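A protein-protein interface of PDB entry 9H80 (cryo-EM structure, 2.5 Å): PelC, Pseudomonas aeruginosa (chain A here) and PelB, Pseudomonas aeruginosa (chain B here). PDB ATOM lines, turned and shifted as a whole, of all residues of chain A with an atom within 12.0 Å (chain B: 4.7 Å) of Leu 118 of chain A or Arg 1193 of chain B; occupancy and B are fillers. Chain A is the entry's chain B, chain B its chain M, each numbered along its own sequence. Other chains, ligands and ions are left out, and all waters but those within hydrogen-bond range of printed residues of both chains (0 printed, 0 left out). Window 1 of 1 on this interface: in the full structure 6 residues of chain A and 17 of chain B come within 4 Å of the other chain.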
ATOM      1  N   GLU A 111      -5.905  -2.200  15.342  1.00  0.00           N
ATOM      2  CA  GLU A 111      -6.138  -2.184  16.776  1.00  0.00           C
ATOM      3  C   GLU A 111      -5.047  -3.001  17.447  1.00  0.00           C
ATOM      4  O   GLU A 111      -4.744  -4.111  17.005  1.00  0.00           O
ATOM      5  CB  GLU A 111      -7.517  -2.753  17.123  1.00  0.00           C
ATOM      6  CG  GLU A 111      -7.963  -2.464  18.545  1.00  0.00           C
ATOM      7  CD  GLU A 111      -9.466  -2.516  18.708  1.00  0.00           C
ATOM      8  OE1 GLU A 111     -10.139  -3.113  17.844  1.00  0.00           O
ATOM      9  OE2 GLU A 111      -9.977  -1.959  19.701  1.00  0.00           O
ATOM     10  N   GLN A 113      -4.323  -3.136  21.557  1.00  0.00           N
ATOM     11  CA  GLN A 113      -4.528  -2.550  22.874  1.00  0.00           C
ATOM     12  C   GLN A 113      -5.328  -3.499  23.748  1.00  0.00           C
ATOM     13  O   GLN A 113      -5.975  -4.431  23.262  1.00  0.00           O
ATOM     14  CB  GLN A 113      -5.245  -1.200  22.774  1.00  0.00           C
ATOM     15  CG  GLN A 113      -6.556  -1.250  22.007  1.00  0.00           C
ATOM     16  CD  GLN A 113      -7.464  -0.085  22.321  1.00  0.00           C
ATOM     17  OE1 GLN A 113      -7.134   1.066  22.040  1.00  0.00           O
ATOM     18  NE2 GLN A 113      -8.617  -0.375  22.911  1.00  0.00           N
ATOM     19  N   TYR A 114      -5.272  -3.243  25.051  1.00  0.00           N
ATOM     20  CA  TYR A 114      -6.175  -3.854  26.010  1.00  0.00           C
ATOM     21  C   TYR A 114      -7.387  -2.952  26.195  1.00  0.00           C
ATOM     22  O   TYR A 114      -7.254  -1.733  26.331  1.00  0.00           O
ATOM     23  CB  TYR A 114      -5.480  -4.071  27.353  1.00  0.00           C
ATOM     24  CG  TYR A 114      -4.516  -5.235  27.384  1.00  0.00           C
ATOM     25  CD1 TYR A 114      -4.977  -6.540  27.428  1.00  0.00           C
ATOM     26  CD2 TYR A 114      -3.144  -5.026  27.388  1.00  0.00           C
ATOM     27  CE1 TYR A 114      -4.105  -7.603  27.461  1.00  0.00           C
ATOM     28  CE2 TYR A 114      -2.264  -6.085  27.424  1.00  0.00           C
ATOM     29  CZ  TYR A 114      -2.752  -7.372  27.462  1.00  0.00           C
ATOM     30  OH  TYR A 114      -1.886  -8.437  27.495  1.00  0.00           O
ATOM     31  N   LYS A 115      -8.572  -3.554  26.187  1.00  0.00           N
ATOM     32  CA  LYS A 115      -9.792  -2.782  26.372  1.00  0.00           C
ATOM     33  C   LYS A 115      -9.917  -2.320  27.819  1.00  0.00           C
ATOM     34  O   LYS A 115      -9.528  -3.020  28.756  1.00  0.00           O
ATOM     35  CB  LYS A 115     -11.011  -3.609  25.970  1.00  0.00           C
ATOM     36  CG  LYS A 115     -11.222  -3.683  24.468  1.00  0.00           C
ATOM     37  CD  LYS A 115     -12.218  -4.758  24.079  1.00  0.00           C
ATOM     38  CE  LYS A 115     -13.630  -4.378  24.475  1.00  0.00           C
ATOM     39  NZ  LYS A 115     -14.617  -5.393  24.030  1.00  0.00           N
ATOM     40  N   ASN A 116     -10.463  -1.120  27.990  1.00  0.00           N
ATOM     41  CA  ASN A 116     -10.610  -0.549  29.323  1.00  0.00           C
ATOM     42  C   ASN A 116     -11.613  -1.350  30.140  1.00  0.00           C
ATOM     43  O   ASN A 116     -12.635  -1.810  29.626  1.00  0.00           O
ATOM     44  CB  ASN A 116     -11.061   0.907  29.231  1.00  0.00           C
ATOM     45  CG  ASN A 116      -9.923   1.849  28.911  1.00  0.00           C
ATOM     46  OD1 ASN A 116      -8.883   1.433  28.404  1.00  0.00           O
ATOM     47  ND2 ASN A 116     -10.113   3.128  29.204  1.00  0.00           N
ATOM     48  N   GLY A 117     -11.311  -1.516  31.424  1.00  0.00           N
ATOM     49  CA  GLY A 117     -12.158  -2.215  32.361  1.00  0.00           C
ATOM     50  C   GLY A 117     -11.352  -3.164  33.210  1.00  0.00           C
ATOM     51  O   GLY A 117     -10.121  -3.218  33.137  1.00  0.00           O
ATOM     52  N   LEU A 118     -12.061  -3.932  34.033  1.00  0.00           N
ATOM     53  CA  LEU A 118     -11.435  -4.918  34.902  1.00  0.00           C
ATOM     54  C   LEU A 118     -11.126  -6.228  34.189  1.00  0.00           C
ATOM     55  O   LEU A 118     -10.467  -7.092  34.776  1.00  0.00           O
ATOM     56  CB  LEU A 118     -12.338  -5.198  36.104  1.00  0.00           C
ATOM     57  CG  LEU A 118     -12.445  -4.100  37.164  1.00  0.00           C
ATOM     58  CD1 LEU A 118     -13.634  -4.366  38.067  1.00  0.00           C
ATOM     59  CD2 LEU A 118     -11.171  -4.002  37.984  1.00  0.00           C
ATOM     60  N   ASP A 119     -11.581  -6.398  32.947  1.00  0.00           N
ATOM     61  CA  ASP A 119     -11.349  -7.647  32.233  1.00  0.00           C
ATOM     62  C   ASP A 119      -9.914  -7.770  31.739  1.00  0.00           C
ATOM     63  O   ASP A 119      -9.395  -8.887  31.645  1.00  0.00           O
ATOM     64  CB  ASP A 119     -12.315  -7.760  31.054  1.00  0.00           C
ATOM     65  CG  ASP A 119     -13.749  -7.963  31.495  1.00  0.00           C
ATOM     66  OD1 ASP A 119     -13.985  -8.070  32.715  1.00  0.00           O
ATOM     67  OD2 ASP A 119     -14.642  -8.017  30.623  1.00  0.00           O
ATOM     68  N   GLY A 120      -9.262  -6.654  31.424  1.00  0.00           N
ATOM     69  CA  GLY A 120      -7.943  -6.707  30.824  1.00  0.00           C
ATOM     70  C   GLY A 120      -7.996  -7.404  29.481  1.00  0.00           C
ATOM     71  O   GLY A 120      -7.176  -8.276  29.184  1.00  0.00           O
ATOM     72  N   GLU A 121      -8.972  -7.025  28.664  1.00  0.00           N
ATOM     73  CA  GLU A 121      -9.287  -7.763  27.451  1.00  0.00           C
ATOM     74  C   GLU A 121      -8.422  -7.270  26.296  1.00  0.00           C
ATOM     75  O   GLU A 121      -8.521  -6.091  25.930  1.00  0.00           O
ATOM     76  CB  GLU A 121     -10.751  -7.593  27.104  1.00  0.00           C
ATOM     77  CG  GLU A 121     -11.404  -8.841  26.582  1.00  0.00           C
ATOM     78  CD  GLU A 121     -12.751  -8.558  25.951  1.00  0.00           C
ATOM     79  OE1 GLU A 121     -12.777  -8.023  24.824  1.00  0.00           O
ATOM     80  OE2 GLU A 121     -13.782  -8.868  26.584  1.00  0.00           O
ATOM     81  N   PRO A 122      -7.574  -8.107  25.693  1.00  0.00           N
ATOM     82  CA  PRO A 122      -6.837  -7.656  24.509  1.00  0.00           C
ATOM     83  C   PRO A 122      -7.745  -7.563  23.293  1.00  0.00           C
ATOM     84  O   PRO A 122      -8.650  -8.377  23.109  1.00  0.00           O
ATOM     85  CB  PRO A 122      -5.763  -8.733  24.325  1.00  0.00           C
ATOM     86  CG  PRO A 122      -6.348  -9.943  24.908  1.00  0.00           C
ATOM     87  CD  PRO A 122      -7.217  -9.494  26.046  1.00  0.00           C
ATOM     88  N   ALA A 123      -7.493  -6.553  22.466  1.00  0.00           N
ATOM     89  CA  ALA A 123      -8.204  -6.359  21.209  1.00  0.00           C
ATOM     90  C   ALA A 123      -7.176  -6.071  20.128  1.00  0.00           C
ATOM     91  O   ALA A 123      -6.456  -5.072  20.208  1.00  0.00           O
ATOM     92  CB  ALA A 123      -9.217  -5.215  21.312  1.00  0.00           C
ATOM     93  N   ALA A 147     -11.322  -9.847  20.089  1.00  0.00           N
ATOM     94  CA  ALA A 147     -11.381  -9.125  21.359  1.00  0.00           C
ATOM     95  C   ALA A 147     -11.788  -9.976  22.553  1.00  0.00           C
ATOM     96  O   ALA A 147     -11.188  -9.844  23.620  1.00  0.00           O
ATOM     97  CB  ALA A 147     -12.350  -7.950  21.249  1.00  0.00           C
ATOM     98  N   GLY A 148     -12.773 -10.855  22.403  1.00  0.00           N
ATOM     99  CA  GLY A 148     -13.478 -11.374  23.562  1.00  0.00           C
ATOM    100  C   GLY A 148     -12.817 -12.504  24.323  1.00  0.00           C
ATOM    101  O   GLY A 148     -13.462 -13.524  24.584  1.00  0.00           O
ATOM    102  N   TRP A 149     -11.543 -12.348  24.697  1.00  0.00           N
ATOM    103  CA  TRP A 149     -10.807 -13.380  25.438  1.00  0.00           C
ATOM    104  C   TRP A 149      -9.949 -12.681  26.490  1.00  0.00           C
ATOM    105  O   TRP A 149      -8.804 -12.312  26.225  1.00  0.00           O
ATOM    106  CB  TRP A 149      -9.965 -14.230  24.500  1.00  0.00           C
ATOM    107  CG  TRP A 149     -10.774 -14.942  23.466  1.00  0.00           C
ATOM    108  CD1 TRP A 149     -11.077 -14.494  22.216  1.00  0.00           C
ATOM    109  CD2 TRP A 149     -11.398 -16.222  23.597  1.00  0.00           C
ATOM    110  NE1 TRP A 149     -11.846 -15.419  21.556  1.00  0.00           N
ATOM    111  CE2 TRP A 149     -12.057 -16.491  22.382  1.00  0.00           C
ATOM    112  CE3 TRP A 149     -11.460 -17.170  24.622  1.00  0.00           C
ATOM    113  CZ2 TRP A 149     -12.769 -17.665  22.165  1.00  0.00           C
ATOM    114  CZ3 TRP A 149     -12.168 -18.335  24.404  1.00  0.00           C
ATOM    115  CH2 TRP A 149     -12.814 -18.574  23.186  1.00  0.00           C
ATOM    116  N   SER A 150     -10.502 -12.529  27.694  1.00  0.00           N
ATOM    117  CA  SER A 150      -9.879 -11.706  28.724  1.00  0.00           C
ATOM    118  C   SER A 150      -8.693 -12.372  29.409  1.00  0.00           C
ATOM    119  O   SER A 150      -7.905 -11.672  30.054  1.00  0.00           O
ATOM    120  CB  SER A 150     -10.917 -11.324  29.779  1.00  0.00           C
ATOM    121  OG  SER A 150     -11.800 -12.401  30.034  1.00  0.00           O
ATOM    122  N   ARG A 151      -8.539 -13.687  29.295  1.00  0.00           N
ATOM    123  CA  ARG A 151      -7.476 -14.395  29.996  1.00  0.00           C
ATOM    124  C   ARG A 151      -6.174 -14.464  29.210  1.00  0.00           C
ATOM    125  O   ARG A 151      -5.166 -14.918  29.762  1.00  0.00           O
ATOM    126  CB  ARG A 151      -7.933 -15.814  30.346  1.00  0.00           C
ATOM    127  CG  ARG A 151      -9.315 -15.878  30.976  1.00  0.00           C
ATOM    128  CD  ARG A 151      -9.466 -17.070  31.907  1.00  0.00           C
ATOM    129  NE  ARG A 151      -8.559 -17.008  33.048  1.00  0.00           N
ATOM    130  CZ  ARG A 151      -8.554 -17.869  34.055  1.00  0.00           C
ATOM    131  NH1 ARG A 151      -9.404 -18.883  34.109  1.00  0.00           N
ATOM    132  NH2 ARG A 151      -7.672 -17.712  35.039  1.00  0.00           N
ATOM    133  N   GLU A 152      -6.161 -14.027  27.955  1.00  0.00           N
ATOM    134  CA  GLU A 152      -4.977 -14.093  27.112  1.00  0.00           C
ATOM    135  C   GLU A 152      -4.316 -12.723  27.026  1.00  0.00           C
ATOM    136  O   GLU A 152      -4.875 -11.704  27.436  1.00  0.00           O
ATOM    137  CB  GLU A 152      -5.338 -14.610  25.715  1.00  0.00           C
ATOM    138  CG  GLU A 152      -5.858 -13.551  24.753  1.00  0.00           C
ATOM    139  CD  GLU A 152      -6.617 -14.140  23.579  1.00  0.00           C
ATOM    140  OE1 GLU A 152      -7.165 -15.255  23.706  1.00  0.00           O
ATOM    141  OE2 GLU A 152      -6.667 -13.485  22.518  1.00  0.00           O
ATOM    142  N   LEU B 852     -14.688   2.039  35.656  1.00  0.00           N
ATOM    143  CA  LEU B 852     -14.444   0.963  34.705  1.00  0.00           C
ATOM    144  C   LEU B 852     -14.022   1.501  33.344  1.00  0.00           C
ATOM    145  O   LEU B 852     -13.280   0.826  32.620  1.00  0.00           O
ATOM    146  CB  LEU B 852     -15.691   0.092  34.565  1.00  0.00           C
ATOM    147  CG  LEU B 852     -16.091  -0.801  35.742  1.00  0.00           C
ATOM    148  CD1 LEU B 852     -17.374  -1.540  35.397  1.00  0.00           C
ATOM    149  CD2 LEU B 852     -15.006  -1.791  36.147  1.00  0.00           C
ATOM    150  N   GLY B 853     -14.469   2.701  32.975  1.00  0.00           N
ATOM    151  CA  GLY B 853     -14.107   3.255  31.687  1.00  0.00           C
ATOM    152  C   GLY B 853     -12.750   3.908  31.616  1.00  0.00           C
ATOM    153  O   GLY B 853     -12.329   4.304  30.527  1.00  0.00           O
ATOM    154  N   LEU B 855      -9.902   2.463  33.430  1.00  0.00           N
ATOM    155  CA  LEU B 855      -8.882   1.503  33.847  1.00  0.00           C
ATOM    156  C   LEU B 855      -8.215   0.925  32.603  1.00  0.00           C
ATOM    157  O   LEU B 855      -8.530  -0.169  32.131  1.00  0.00           O
ATOM    158  CB  LEU B 855      -9.505   0.411  34.711  1.00  0.00           C
ATOM    159  CG  LEU B 855      -8.575  -0.560  35.443  1.00  0.00           C
ATOM    160  CD1 LEU B 855      -7.503   0.160  36.249  1.00  0.00           C
ATOM    161  CD2 LEU B 855      -9.391  -1.470  36.339  1.00  0.00           C
ATOM    162  N   ARG B 868      -8.830   0.369  40.187  1.00  0.00           N
ATOM    163  CA  ARG B 868      -9.121  -1.049  40.352  1.00  0.00           C
ATOM    164  C   ARG B 868      -9.705  -1.324  41.730  1.00  0.00           C
ATOM    165  O   ARG B 868     -10.699  -2.047  41.864  1.00  0.00           O
ATOM    166  CB  ARG B 868      -7.850  -1.870  40.128  1.00  0.00           C
ATOM    167  CG  ARG B 868      -8.090  -3.358  39.943  1.00  0.00           C
ATOM    168  CD  ARG B 868      -6.807  -4.155  40.099  1.00  0.00           C
ATOM    169  NE  ARG B 868      -5.785  -3.744  39.139  1.00  0.00           N
ATOM    170  CZ  ARG B 868      -4.649  -3.118  39.428  1.00  0.00           C
ATOM    171  NH1 ARG B 868      -4.335  -2.764  40.665  1.00  0.00           N
ATOM    172  NH2 ARG B 868      -3.804  -2.829  38.444  1.00  0.00           N
ATOM    173  N   ALA B 871     -13.286   0.165  41.946  1.00  0.00           N
ATOM    174  CA  ALA B 871     -14.213  -0.646  41.169  1.00  0.00           C
ATOM    175  C   ALA B 871     -14.514  -1.956  41.879  1.00  0.00           C
ATOM    176  O   ALA B 871     -15.667  -2.397  41.921  1.00  0.00           O
ATOM    177  CB  ALA B 871     -13.640  -0.905  39.777  1.00  0.00           C
ATOM    178  N   LEU B 875     -18.187  -3.055  43.185  1.00  0.00           N
ATOM    179  CA  LEU B 875     -18.766  -4.311  42.727  1.00  0.00           C
ATOM    180  C   LEU B 875     -19.097  -5.225  43.896  1.00  0.00           C
ATOM    181  O   LEU B 875     -20.067  -5.987  43.831  1.00  0.00           O
ATOM    182  CB  LEU B 875     -17.805  -5.007  41.764  1.00  0.00           C
ATOM    183  CG  LEU B 875     -17.655  -4.406  40.363  1.00  0.00           C
ATOM    184  CD1 LEU B 875     -16.643  -5.209  39.569  1.00  0.00           C
ATOM    185  CD2 LEU B 875     -18.987  -4.346  39.625  1.00  0.00           C
ATOM    186  N   ARG B1190     -20.122 -11.661  35.120  1.00  0.00           N
ATOM    187  CA  ARG B1190     -20.207 -10.249  35.465  1.00  0.00           C
ATOM    188  C   ARG B1190     -20.605  -9.434  34.244  1.00  0.00           C
ATOM    189  O   ARG B1190     -20.060  -9.634  33.154  1.00  0.00           O
ATOM    190  CB  ARG B1190     -18.866  -9.755  36.012  1.00  0.00           C
ATOM    191  CG  ARG B1190     -18.833  -8.281  36.367  1.00  0.00           C
ATOM    192  CD  ARG B1190     -17.520  -7.908  37.026  1.00  0.00           C
ATOM    193  NE  ARG B1190     -16.487  -7.611  36.042  1.00  0.00           N
ATOM    194  CZ  ARG B1190     -16.365  -6.460  35.393  1.00  0.00           C
ATOM    195  NH1 ARG B1190     -17.201  -5.455  35.597  1.00  0.00           N
ATOM    196  NH2 ARG B1190     -15.379  -6.314  34.514  1.00  0.00           N
ATOM    197  N   GLY B1192     -20.116  -6.071  32.559  1.00  0.00           N
ATOM    198  CA  GLY B1192     -19.198  -4.952  32.589  1.00  0.00           C
ATOM    199  C   GLY B1192     -18.050  -5.152  31.627  1.00  0.00           C
ATOM    200  O   GLY B1192     -17.768  -6.251  31.155  1.00  0.00           O
ATOM    201  N   ARG B1193     -17.364  -4.053  31.335  1.00  0.00           N
ATOM    202  CA  ARG B1193     -16.242  -4.064  30.410  1.00  0.00           C
ATOM    203  C   ARG B1193     -14.975  -4.594  31.078  1.00  0.00           C
ATOM    204  O   ARG B1193     -14.975  -4.916  32.266  1.00  0.00           O
ATOM    205  CB  ARG B1193     -16.000  -2.661  29.857  1.00  0.00           C
ATOM    206  CG  ARG B1193     -16.006  -1.577  30.915  1.00  0.00           C
ATOM    207  CD  ARG B1193     -16.154  -0.198  30.305  1.00  0.00           C
ATOM    208  NE  ARG B1193     -15.208   0.027  29.220  1.00  0.00           N
ATOM    209  CZ  ARG B1193     -15.097   1.166  28.551  1.00  0.00           C
ATOM    210  NH1 ARG B1193     -15.850   2.213  28.841  1.00  0.00           N
ATOM    211  NH2 ARG B1193     -14.209   1.256  27.567  1.00  0.00           N
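The backbone carbonyl oxygen (O) of Leu 852 of chain B lies close to the backbone NH (N) of Gly 117 of chain A, at 3.3 Å.
O of Gly 853 of chain B is in hydrogen-bond range of ND2 of Asn 116 of chain A.
The backbone NH of Gly 117 of chain A lies within hydrogen-bond range of the backbone carbonyl oxygen of Leu 855 of chain B, at 3.2 Å.
NH2 of Arg 1190 of chain B lies within salt-bridge range of OD1 of Asp 119 of chain A (2.9 Å).
The guanidinium group of Arg 1193 of chain B sits at hydrogen-bond distance from the backbone carbonyl oxygen of Asn 116 of chain A (3.2 Å).
OD1 of Asp 119 of chain A lies close to O of Arg 1193 of chain B (3.3 Å).
NH2 of Arg 1190 of chain B is in hydrogen-bond range of O of Arg 1193 of chain B (2.7 Å).
Leu 852 of chain B touches Asn 116 of chain A.
Leu 855 of chain B touches Asn 116 of chain A (O to CA, 3.5 Å).
CD2 of Leu 852 of chain B touches CD1 of Leu 118 of chain A (3.5 Å).
Leu 118 of chain A touches Leu 855 of chain B (CD2 to CD2, 3.5 Å).
Arg 868 of chain B touches Leu 118 of chain A (CG to CD2, 3.7 Å).
CD1 of Leu 118 of chain A touches CB of Ala 871 of chain B, at 3.9 Å.
Leu 875 of chain B touches Leu 118 of chain A (CD1 to CD1, 3.5 Å).
Arg 1190 of chain B touches Leu 118 of chain A (NH2 to CB, 3.6 Å).
Leu 118 of chain A touches Arg 1193 of chain B (N to O, 3.5 Å).
Asp 119 of chain A touches Gly 1192 of chain B (OD2 to O, 3.6 Å).
Of the printed residues of chain B, Asn 116 of chain A touches Leu 852 (3.7 Å), Gly 853 (2.8 Å), Leu 855 (3.5 Å) and Arg 1193 (3.2 Å).
Printed residues of chain B within 4 Å of Gly 117 of chain A: Leu 852 (3.3 Å), Leu 855 (3.2 Å) and Arg 1193 (3.9 Å).
Leu 118 of chain A touches seven residues of chain B.
Of the printed residues of chain B, Asp 119 of chain A touches Arg 1190, Gly 1192 and Arg 1193.
Of chain A, only Asn 116, Gly 117 and Leu 118 come within 4 Å of Leu 852 of chain B.
Of chain A, only Asn 116 (3.5 Å), Gly 117 (3.2 Å) and Leu 118 (3.5 Å) come within 4 Å of Leu 855 of chain B.
Arg 868 of chain B touches just one residue of chain A: Leu 118.
Ala 871 of chain B touches just one residue of chain A: Leu 118 (3.9 Å).
Of the printed residues of chain A, Leu 875 of chain B touches Leu 118 (3.5 Å).
Of the printed residues of chain A, Arg 1190 of chain B touches Leu 118 and Asp 119.
Of chain A, only Asp 119 (3.6 Å) comes within 4 Å of Gly 1192 of chain B.
Of chain A, only Asn 116 (3.2 Å), Gly 117 (3.9 Å), Leu 118 (3.5 Å) and Asp 119 (3.3 Å) come within 4 Å of Arg 1193 of chain B.
The nearest printed residue of chain B that does not touch Leu 118 of chain A is Gly 1192 of chain B (6.6 Å).
Printed residues of chain A that touch a printed residue of chain B: Asn 116, Gly 117, Leu 118 and Asp 119.
Hydrophobic or aromatic side chains of chain A that line the printed part of chain B: Leu 118.
Along chain A the printed residues that touch a printed residue of chain B span positions 116 to 119.
Among the printed residues, Asp or Glu carboxylates within 4 Å of a Lys or Arg side-chain nitrogen of the other chain: Asp 119 of chain A with Arg 1190 of chain B (2.9 Å).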
